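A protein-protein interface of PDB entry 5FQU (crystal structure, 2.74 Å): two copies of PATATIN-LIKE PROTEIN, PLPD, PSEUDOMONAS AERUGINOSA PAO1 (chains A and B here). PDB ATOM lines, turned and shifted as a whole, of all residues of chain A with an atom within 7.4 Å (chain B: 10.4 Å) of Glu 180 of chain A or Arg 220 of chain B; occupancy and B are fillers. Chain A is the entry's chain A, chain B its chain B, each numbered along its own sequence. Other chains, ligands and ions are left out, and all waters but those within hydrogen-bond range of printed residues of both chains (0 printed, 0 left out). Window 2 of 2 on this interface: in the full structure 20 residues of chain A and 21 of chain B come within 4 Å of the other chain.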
ATOM      1  N   ASP A 148     -23.597   0.161 -30.346  1.00  0.00           N
ATOM      2  CA  ASP A 148     -22.372   0.935 -30.080  1.00  0.00           C
ATOM      3  C   ASP A 148     -22.162   0.976 -28.584  1.00  0.00           C
ATOM      4  O   ASP A 148     -22.854   1.714 -27.847  1.00  0.00           O
ATOM      5  CB  ASP A 148     -22.513   2.374 -30.617  1.00  0.00           C
ATOM      6  CG  ASP A 148     -21.182   3.198 -30.572  1.00  0.00           C
ATOM      7  OD1 ASP A 148     -20.088   2.686 -30.186  1.00  0.00           O
ATOM      8  OD2 ASP A 148     -21.259   4.386 -30.967  1.00  0.00           O
ATOM      9  N   ILE A 149     -21.213   0.179 -28.121  1.00  0.00           N
ATOM     10  CA  ILE A 149     -21.028   0.010 -26.686  1.00  0.00           C
ATOM     11  C   ILE A 149     -20.513   1.281 -26.000  1.00  0.00           C
ATOM     12  O   ILE A 149     -20.775   1.509 -24.834  1.00  0.00           O
ATOM     13  CB  ILE A 149     -20.127  -1.201 -26.387  1.00  0.00           C
ATOM     14  CG1 ILE A 149     -20.231  -1.591 -24.918  1.00  0.00           C
ATOM     15  CG2 ILE A 149     -18.682  -0.939 -26.769  1.00  0.00           C
ATOM     16  CD1 ILE A 149     -21.651  -1.836 -24.435  1.00  0.00           C
ATOM     17  N   ALA A 150     -19.842   2.142 -26.754  1.00  0.00           N
ATOM     18  CA  ALA A 150     -19.387   3.436 -26.252  1.00  0.00           C
ATOM     19  C   ALA A 150     -20.525   4.430 -25.979  1.00  0.00           C
ATOM     20  O   ALA A 150     -20.407   5.247 -25.089  1.00  0.00           O
ATOM     21  CB  ALA A 150     -18.409   4.046 -27.234  1.00  0.00           C
ATOM     22  N   THR A 151     -21.599   4.390 -26.763  1.00  0.00           N
ATOM     23  CA  THR A 151     -22.653   5.407 -26.685  1.00  0.00           C
ATOM     24  C   THR A 151     -24.042   4.845 -26.462  1.00  0.00           C
ATOM     25  O   THR A 151     -24.983   5.605 -26.327  1.00  0.00           O
ATOM     26  CB  THR A 151     -22.705   6.256 -27.977  1.00  0.00           C
ATOM     27  OG1 THR A 151     -23.397   5.559 -29.007  1.00  0.00           O
ATOM     28  CG2 THR A 151     -21.293   6.570 -28.491  1.00  0.00           C
ATOM     29  N   GLN A 164     -18.782  -9.460 -41.716  1.00  0.00           N
ATOM     30  CA  GLN A 164     -18.320  -8.572 -40.650  1.00  0.00           C
ATOM     31  C   GLN A 164     -19.543  -7.994 -39.913  1.00  0.00           C
ATOM     32  O   GLN A 164     -19.614  -8.084 -38.695  1.00  0.00           O
ATOM     33  CB  GLN A 164     -17.411  -7.512 -41.285  1.00  0.00           C
ATOM     34  CG  GLN A 164     -16.890  -6.422 -40.385  1.00  0.00           C
ATOM     35  CD  GLN A 164     -16.538  -5.137 -41.157  1.00  0.00           C
ATOM     36  OE1 GLN A 164     -17.362  -4.550 -41.923  1.00  0.00           O
ATOM     37  NE2 GLN A 164     -15.316  -4.670 -40.937  1.00  0.00           N
ATOM     38  N   ALA A 168     -20.806  -8.595 -36.025  1.00  0.00           N
ATOM     39  CA  ALA A 168     -21.100  -7.525 -35.038  1.00  0.00           C
ATOM     40  C   ALA A 168     -22.366  -7.795 -34.273  1.00  0.00           C
ATOM     41  O   ALA A 168     -22.369  -7.787 -33.051  1.00  0.00           O
ATOM     42  CB  ALA A 168     -21.211  -6.163 -35.696  1.00  0.00           C
ATOM     43  N   ALA A 177     -15.658 -11.279 -28.292  1.00  0.00           N
ATOM     44  CA  ALA A 177     -15.121  -9.918 -28.179  1.00  0.00           C
ATOM     45  C   ALA A 177     -15.888  -8.964 -29.078  1.00  0.00           C
ATOM     46  O   ALA A 177     -16.401  -9.358 -30.123  1.00  0.00           O
ATOM     47  CB  ALA A 177     -13.652  -9.898 -28.551  1.00  0.00           C
ATOM     48  N   PRO A 178     -15.982  -7.704 -28.683  1.00  0.00           N
ATOM     49  CA  PRO A 178     -16.681  -6.770 -29.562  1.00  0.00           C
ATOM     50  C   PRO A 178     -15.878  -6.557 -30.837  1.00  0.00           C
ATOM     51  O   PRO A 178     -14.740  -7.007 -30.912  1.00  0.00           O
ATOM     52  CB  PRO A 178     -16.721  -5.477 -28.749  1.00  0.00           C
ATOM     53  CG  PRO A 178     -16.385  -5.867 -27.363  1.00  0.00           C
ATOM     54  CD  PRO A 178     -15.521  -7.078 -27.444  1.00  0.00           C
ATOM     55  N   VAL A 179     -16.455  -5.885 -31.828  1.00  0.00           N
ATOM     56  CA  VAL A 179     -15.751  -5.670 -33.091  1.00  0.00           C
ATOM     57  C   VAL A 179     -15.680  -4.179 -33.400  1.00  0.00           C
ATOM     58  O   VAL A 179     -16.590  -3.443 -32.998  1.00  0.00           O
ATOM     59  CB  VAL A 179     -16.372  -6.469 -34.289  1.00  0.00           C
ATOM     60  CG1 VAL A 179     -16.404  -7.947 -33.981  1.00  0.00           C
ATOM     61  CG2 VAL A 179     -17.769  -6.005 -34.637  1.00  0.00           C
ATOM     62  N   GLU A 180     -14.615  -3.771 -34.122  1.00  0.00           N
ATOM     63  CA  GLU A 180     -14.350  -2.371 -34.507  1.00  0.00           C
ATOM     64  C   GLU A 180     -14.602  -2.084 -35.982  1.00  0.00           C
ATOM     65  O   GLU A 180     -13.812  -2.485 -36.812  1.00  0.00           O
ATOM     66  CB  GLU A 180     -12.904  -2.025 -34.187  1.00  0.00           C
ATOM     67  CG  GLU A 180     -12.651  -1.995 -32.698  1.00  0.00           C
ATOM     68  CD  GLU A 180     -11.217  -1.693 -32.333  1.00  0.00           C
ATOM     69  OE1 GLU A 180     -10.443  -1.225 -33.197  1.00  0.00           O
ATOM     70  OE2 GLU A 180     -10.877  -1.925 -31.158  1.00  0.00           O
ATOM     71  N   ILE A 181     -15.657  -1.326 -36.290  1.00  0.00           N
ATOM     72  CA  ILE A 181     -16.112  -1.099 -37.679  1.00  0.00           C
ATOM     73  C   ILE A 181     -16.387   0.396 -38.011  1.00  0.00           C
ATOM     74  O   ILE A 181     -17.496   0.924 -37.830  1.00  0.00           O
ATOM     75  CB  ILE A 181     -17.362  -1.974 -37.973  1.00  0.00           C
ATOM     76  CG1 ILE A 181     -17.017  -3.461 -37.811  1.00  0.00           C
ATOM     77  CG2 ILE A 181     -17.949  -1.719 -39.367  1.00  0.00           C
ATOM     78  CD1 ILE A 181     -18.229  -4.366 -37.919  1.00  0.00           C
ATOM     79  N   ARG A 184     -16.686   3.003 -34.241  1.00  0.00           N
ATOM     80  CA  ARG A 184     -17.595   2.346 -33.309  1.00  0.00           C
ATOM     81  C   ARG A 184     -17.054   0.992 -32.836  1.00  0.00           C
ATOM     82  O   ARG A 184     -16.635   0.173 -33.647  1.00  0.00           O
ATOM     83  CB  ARG A 184     -18.949   2.182 -33.979  1.00  0.00           C
ATOM     84  CG  ARG A 184     -19.352   3.389 -34.815  1.00  0.00           C
ATOM     85  CD  ARG A 184     -20.789   3.297 -35.309  1.00  0.00           C
ATOM     86  NE  ARG A 184     -21.711   4.111 -34.503  1.00  0.00           N
ATOM     87  CZ  ARG A 184     -22.629   4.959 -34.987  1.00  0.00           C
ATOM     88  NH1 ARG A 184     -22.801   5.128 -36.305  1.00  0.00           N
ATOM     89  NH2 ARG A 184     -23.407   5.644 -34.147  1.00  0.00           N
ATOM     90  N   LEU A 185     -16.998   0.795 -31.518  1.00  0.00           N
ATOM     91  CA  LEU A 185     -16.839  -0.544 -30.925  1.00  0.00           C
ATOM     92  C   LEU A 185     -18.210  -1.190 -30.691  1.00  0.00           C
ATOM     93  O   LEU A 185     -19.035  -0.639 -29.958  1.00  0.00           O
ATOM     94  CB  LEU A 185     -16.089  -0.470 -29.595  1.00  0.00           C
ATOM     95  CG  LEU A 185     -15.677  -1.819 -29.007  1.00  0.00           C
ATOM     96  CD1 LEU A 185     -14.690  -2.500 -29.922  1.00  0.00           C
ATOM     97  CD2 LEU A 185     -15.069  -1.653 -27.625  1.00  0.00           C
ATOM     98  N   LEU A 186     -18.415  -2.378 -31.265  1.00  0.00           N
ATOM     99  CA  LEU A 186     -19.751  -2.919 -31.503  1.00  0.00           C
ATOM    100  C   LEU A 186     -20.038  -4.255 -30.836  1.00  0.00           C
ATOM    101  O   LEU A 186     -19.186  -5.162 -30.837  1.00  0.00           O
ATOM    102  CB  LEU A 186     -19.953  -3.079 -32.990  1.00  0.00           C
ATOM    103  CG  LEU A 186     -20.050  -1.741 -33.706  1.00  0.00           C
ATOM    104  CD1 LEU A 186     -19.708  -1.974 -35.149  1.00  0.00           C
ATOM    105  CD2 LEU A 186     -21.427  -1.077 -33.600  1.00  0.00           C
ATOM    106  N   PRO B 216     -22.153   8.739 -15.842  1.00  0.00           N
ATOM    107  CA  PRO B 216     -21.490   8.983 -17.111  1.00  0.00           C
ATOM    108  C   PRO B 216     -21.122   7.665 -17.767  1.00  0.00           C
ATOM    109  O   PRO B 216     -20.786   6.720 -17.034  1.00  0.00           O
ATOM    110  CB  PRO B 216     -20.245   9.733 -16.687  1.00  0.00           C
ATOM    111  CG  PRO B 216     -19.933   9.174 -15.335  1.00  0.00           C
ATOM    112  CD  PRO B 216     -21.257   8.908 -14.691  1.00  0.00           C
ATOM    113  N   LEU B 217     -21.214   7.595 -19.105  1.00  0.00           N
ATOM    114  CA  LEU B 217     -20.760   6.404 -19.869  1.00  0.00           C
ATOM    115  C   LEU B 217     -19.239   6.404 -19.944  1.00  0.00           C
ATOM    116  O   LEU B 217     -18.649   7.474 -20.003  1.00  0.00           O
ATOM    117  CB  LEU B 217     -21.323   6.389 -21.293  1.00  0.00           C
ATOM    118  CG  LEU B 217     -22.795   6.015 -21.511  1.00  0.00           C
ATOM    119  CD1 LEU B 217     -23.678   7.052 -20.873  1.00  0.00           C
ATOM    120  CD2 LEU B 217     -23.138   5.910 -22.989  1.00  0.00           C
ATOM    121  N   ARG B 218     -18.600   5.229 -19.935  1.00  0.00           N
ATOM    122  CA  ARG B 218     -17.137   5.162 -20.093  1.00  0.00           C
ATOM    123  C   ARG B 218     -16.752   5.442 -21.534  1.00  0.00           C
ATOM    124  O   ARG B 218     -17.511   5.133 -22.454  1.00  0.00           O
ATOM    125  CB  ARG B 218     -16.585   3.810 -19.668  1.00  0.00           C
ATOM    126  CG  ARG B 218     -16.508   3.655 -18.168  1.00  0.00           C
ATOM    127  CD  ARG B 218     -15.936   2.303 -17.721  1.00  0.00           C
ATOM    128  NE  ARG B 218     -14.471   2.300 -17.605  1.00  0.00           N
ATOM    129  CZ  ARG B 218     -13.754   2.984 -16.701  1.00  0.00           C
ATOM    130  NH1 ARG B 218     -14.339   3.777 -15.810  1.00  0.00           N
ATOM    131  NH2 ARG B 218     -12.433   2.891 -16.697  1.00  0.00           N
ATOM    132  N   ASP B 219     -15.594   6.062 -21.741  1.00  0.00           N
ATOM    133  CA  ASP B 219     -15.170   6.402 -23.095  1.00  0.00           C
ATOM    134  C   ASP B 219     -14.575   5.193 -23.751  1.00  0.00           C
ATOM    135  O   ASP B 219     -14.122   4.273 -23.081  1.00  0.00           O
ATOM    136  CB  ASP B 219     -14.157   7.546 -23.088  1.00  0.00           C
ATOM    137  CG  ASP B 219     -14.803   8.877 -22.797  1.00  0.00           C
ATOM    138  OD1 ASP B 219     -15.615   9.323 -23.631  1.00  0.00           O
ATOM    139  OD2 ASP B 219     -14.539   9.457 -21.727  1.00  0.00           O
ATOM    140  N   ARG B 220     -14.556   5.208 -25.069  1.00  0.00           N
ATOM    141  CA  ARG B 220     -14.008   4.091 -25.841  1.00  0.00           C
ATOM    142  C   ARG B 220     -12.631   3.637 -25.294  1.00  0.00           C
ATOM    143  O   ARG B 220     -12.380   2.439 -25.132  1.00  0.00           O
ATOM    144  CB  ARG B 220     -13.988   4.454 -27.352  1.00  0.00           C
ATOM    145  CG  ARG B 220     -13.089   3.629 -28.277  1.00  0.00           C
ATOM    146  CD  ARG B 220     -13.544   2.191 -28.483  1.00  0.00           C
ATOM    147  NE  ARG B 220     -12.478   1.375 -29.077  1.00  0.00           N
ATOM    148  CZ  ARG B 220     -11.663   0.544 -28.414  1.00  0.00           C
ATOM    149  NH1 ARG B 220     -11.751   0.355 -27.101  1.00  0.00           N
ATOM    150  NH2 ARG B 220     -10.736  -0.127 -29.084  1.00  0.00           N
ATOM    151  N   LYS B 221     -11.772   4.589 -24.952  1.00  0.00           N
ATOM    152  CA  LYS B 221     -10.406   4.251 -24.532  1.00  0.00           C
ATOM    153  C   LYS B 221     -10.355   3.526 -23.176  1.00  0.00           C
ATOM    154  O   LYS B 221      -9.382   2.850 -22.862  1.00  0.00           O
ATOM    155  CB  LYS B 221      -9.502   5.492 -24.536  1.00  0.00           C
ATOM    156  CG  LYS B 221     -10.141   6.729 -23.929  1.00  0.00           C
ATOM    157  CD  LYS B 221      -9.112   7.750 -23.466  1.00  0.00           C
ATOM    158  CE  LYS B 221      -9.770   8.882 -22.686  1.00  0.00           C
ATOM    159  NZ  LYS B 221      -8.956  10.118 -22.787  1.00  0.00           N
ATOM    160  N   ASP B 222     -11.414   3.640 -22.388  1.00  0.00           N
ATOM    161  CA  ASP B 222     -11.447   3.037 -21.060  1.00  0.00           C
ATOM    162  C   ASP B 222     -12.100   1.672 -21.061  1.00  0.00           C
ATOM    163  O   ASP B 222     -11.946   0.925 -20.109  1.00  0.00           O
ATOM    164  CB  ASP B 222     -12.195   3.943 -20.084  1.00  0.00           C
ATOM    165  CG  ASP B 222     -11.460   5.242 -19.812  1.00  0.00           C
ATOM    166  OD1 ASP B 222     -10.345   5.443 -20.353  1.00  0.00           O
ATOM    167  OD2 ASP B 222     -12.008   6.063 -19.047  1.00  0.00           O
ATOM    168  N   LEU B 223     -12.826   1.338 -22.116  1.00  0.00           N
ATOM    169  CA  LEU B 223     -13.410   0.003 -22.233  1.00  0.00           C
ATOM    170  C   LEU B 223     -12.349  -1.052 -22.568  1.00  0.00           C
ATOM    171  O   LEU B 223     -12.258  -1.500 -23.692  1.00  0.00           O
ATOM    172  CB  LEU B 223     -14.517   0.013 -23.301  1.00  0.00           C
ATOM    173  CG  LEU B 223     -15.730   0.886 -22.951  1.00  0.00           C
ATOM    174  CD1 LEU B 223     -16.719   1.028 -24.106  1.00  0.00           C
ATOM    175  CD2 LEU B 223     -16.427   0.328 -21.721  1.00  0.00           C
ATOM    176  N   SER B 224     -11.558  -1.457 -21.581  1.00  0.00           N
ATOM    177  CA  SER B 224     -10.520  -2.467 -21.785  1.00  0.00           C
ATOM    178  C   SER B 224     -11.107  -3.869 -21.667  1.00  0.00           C
ATOM    179  O   SER B 224     -11.121  -4.620 -22.650  1.00  0.00           O
ATOM    180  CB  SER B 224      -9.383  -2.307 -20.767  1.00  0.00           C
ATOM    181  OG  SER B 224      -8.808  -1.018 -20.848  1.00  0.00           O
ATOM    182  N   THR B 225     -11.601  -4.210 -20.475  1.00  0.00           N
ATOM    183  CA  THR B 225     -11.983  -5.587 -20.156  1.00  0.00           C
ATOM    184  C   THR B 225     -13.484  -5.904 -20.332  1.00  0.00           C
ATOM    185  O   THR B 225     -14.327  -5.036 -20.628  1.00  0.00           O
ATOM    186  CB  THR B 225     -11.573  -5.971 -18.720  1.00  0.00           C
ATOM    187  OG1 THR B 225     -12.307  -5.177 -17.781  1.00  0.00           O
ATOM    188  CG2 THR B 225     -10.065  -5.798 -18.515  1.00  0.00           C
ATOM    189  N   ASP B 228     -15.687  -4.201 -17.909  1.00  0.00           N
ATOM    190  CA  ASP B 228     -15.942  -2.836 -18.377  1.00  0.00           C
ATOM    191  C   ASP B 228     -17.127  -2.745 -19.335  1.00  0.00           C
ATOM    192  O   ASP B 228     -17.945  -1.842 -19.240  1.00  0.00           O
ATOM    193  CB  ASP B 228     -14.693  -2.238 -19.051  1.00  0.00           C
ATOM    194  CG  ASP B 228     -13.666  -1.729 -18.048  1.00  0.00           C
ATOM    195  OD1 ASP B 228     -13.058  -2.551 -17.340  1.00  0.00           O
ATOM    196  OD2 ASP B 228     -13.475  -0.498 -17.962  1.00  0.00           O
ATOM    197  N   VAL B 229     -17.231  -3.691 -20.256  1.00  0.00           N
ATOM    198  CA  VAL B 229     -18.326  -3.660 -21.218  1.00  0.00           C
ATOM    199  C   VAL B 229     -19.662  -3.858 -20.507  1.00  0.00           C
ATOM    200  O   VAL B 229     -20.675  -3.282 -20.896  1.00  0.00           O
ATOM    201  CB  VAL B 229     -18.136  -4.711 -22.337  1.00  0.00           C
ATOM    202  CG1 VAL B 229     -19.381  -4.834 -23.217  1.00  0.00           C
ATOM    203  CG2 VAL B 229     -16.911  -4.376 -23.183  1.00  0.00           C
ATOM    204  N   GLN B 232     -20.922  -0.998 -18.459  1.00  0.00           N
ATOM    205  CA  GLN B 232     -21.412  -0.034 -19.422  1.00  0.00           C
ATOM    206  C   GLN B 232     -22.871  -0.338 -19.774  1.00  0.00           C
ATOM    207  O   GLN B 232     -23.707   0.568 -19.878  1.00  0.00           O
ATOM    208  CB  GLN B 232     -20.517  -0.073 -20.670  1.00  0.00           C
ATOM    209  CG  GLN B 232     -20.895   0.869 -21.807  1.00  0.00           C
ATOM    210  CD  GLN B 232     -20.513   2.311 -21.551  1.00  0.00           C
ATOM    211  OE1 GLN B 232     -19.373   2.619 -21.218  1.00  0.00           O
ATOM    212  NE2 GLN B 232     -21.485   3.206 -21.684  1.00  0.00           N
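O of Leu 185 of chain A is in hydrogen-bond range of N of Ile 149 of chain A, 3.0 Å away.
The guanidinium group (NH2) of Arg 218 of chain B is in salt-bridge range of the side-chain carboxylate (OD2) of Asp 222 of chain B, 3.97 Å away.
The side-chain carboxylate of Asp 148 of chain A lies close to the backbone NH of Ala 150 of chain A (3.5 Å).
The side-chain carboxylate of Asp 148 of chain A lies within hydrogen-bond range of the side-chain hydroxyl of Thr 151 of chain A.
The backbone NH (N) of Arg 218 of chain B lies within hydrogen-bond range of the side-chain amide oxygen (OE1) of Gln 232 of chain B (3.0 Å).
The guanidinium group (NE) of Arg 218 of chain B lies within salt-bridge range of the side-chain carboxylate (OD2) of Asp 228 of chain B, at 3.0 Å.
Glu 180 of chain A touches one residue of chain B.
Of chain A, only Glu 180 and Leu 185 come within 4 Å of Arg 220 of chain B.
Ala 150 of chain A touches just these residues of chain B: Leu 217 and Arg 218.
No residue of chain B comes within 4 Å of Ile 181 of chain A.
Of the printed residues of chain A, Val 229 of chain B touches Ile 149.
Of the printed residues of chain A, Arg 218 of chain B touches Ala 150.
Ala 168 of chain A touches none of the printed residues of chain B.
Ser 224 of chain B touches none of the printed residues of chain A.
The nearest residue of chain B that does not touch Glu 180 of chain A is Leu 223 of chain B (7.6 Å).
The nearest residue of chain A that does not touch Arg 220 of chain B is Ala 150 of chain A (4.4 Å).
The side-chain carboxylate (OE2) of Glu 180 of chain A lies within salt-bridge range of the guanidinium group (NH2) of Arg 220 of chain B (2.7 Å).
Among the printed residues, pairs that only touch across the chains: Ile 149 of chain A with Gln 232 of chain B, Ala 150 of chain A with Leu 217 of chain B, Thr 151 of chain A with Leu 217 of chain B, Ile 149 of chain A with Val 229 of chain B, Leu 185 of chain A with Arg 220 of chain B, Ile 149 of chain A with Leu 223 of chain B and Ala 150 of chain A with Arg 218 of chain B.
No position is printed for both chains.
Of the 8 pairs that touch across the chains among the printed residues, none has its exchanged pair printed and touching as well.
Printed residues of chain A that touch a printed residue of chain B: Ile 149, Ala 150, Thr 151, Glu 180 and Leu 185.
Hydrophobic or aromatic side chains of chain A that line the printed part of chain B: Ile 149 and Leu 185.
Among the printed residues, Asp or Glu carboxylates within 4 Å of a Lys or Arg side-chain nitrogen of the other chain: Glu 180 of chain A with Arg 220 of chain B (2.7 Å).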
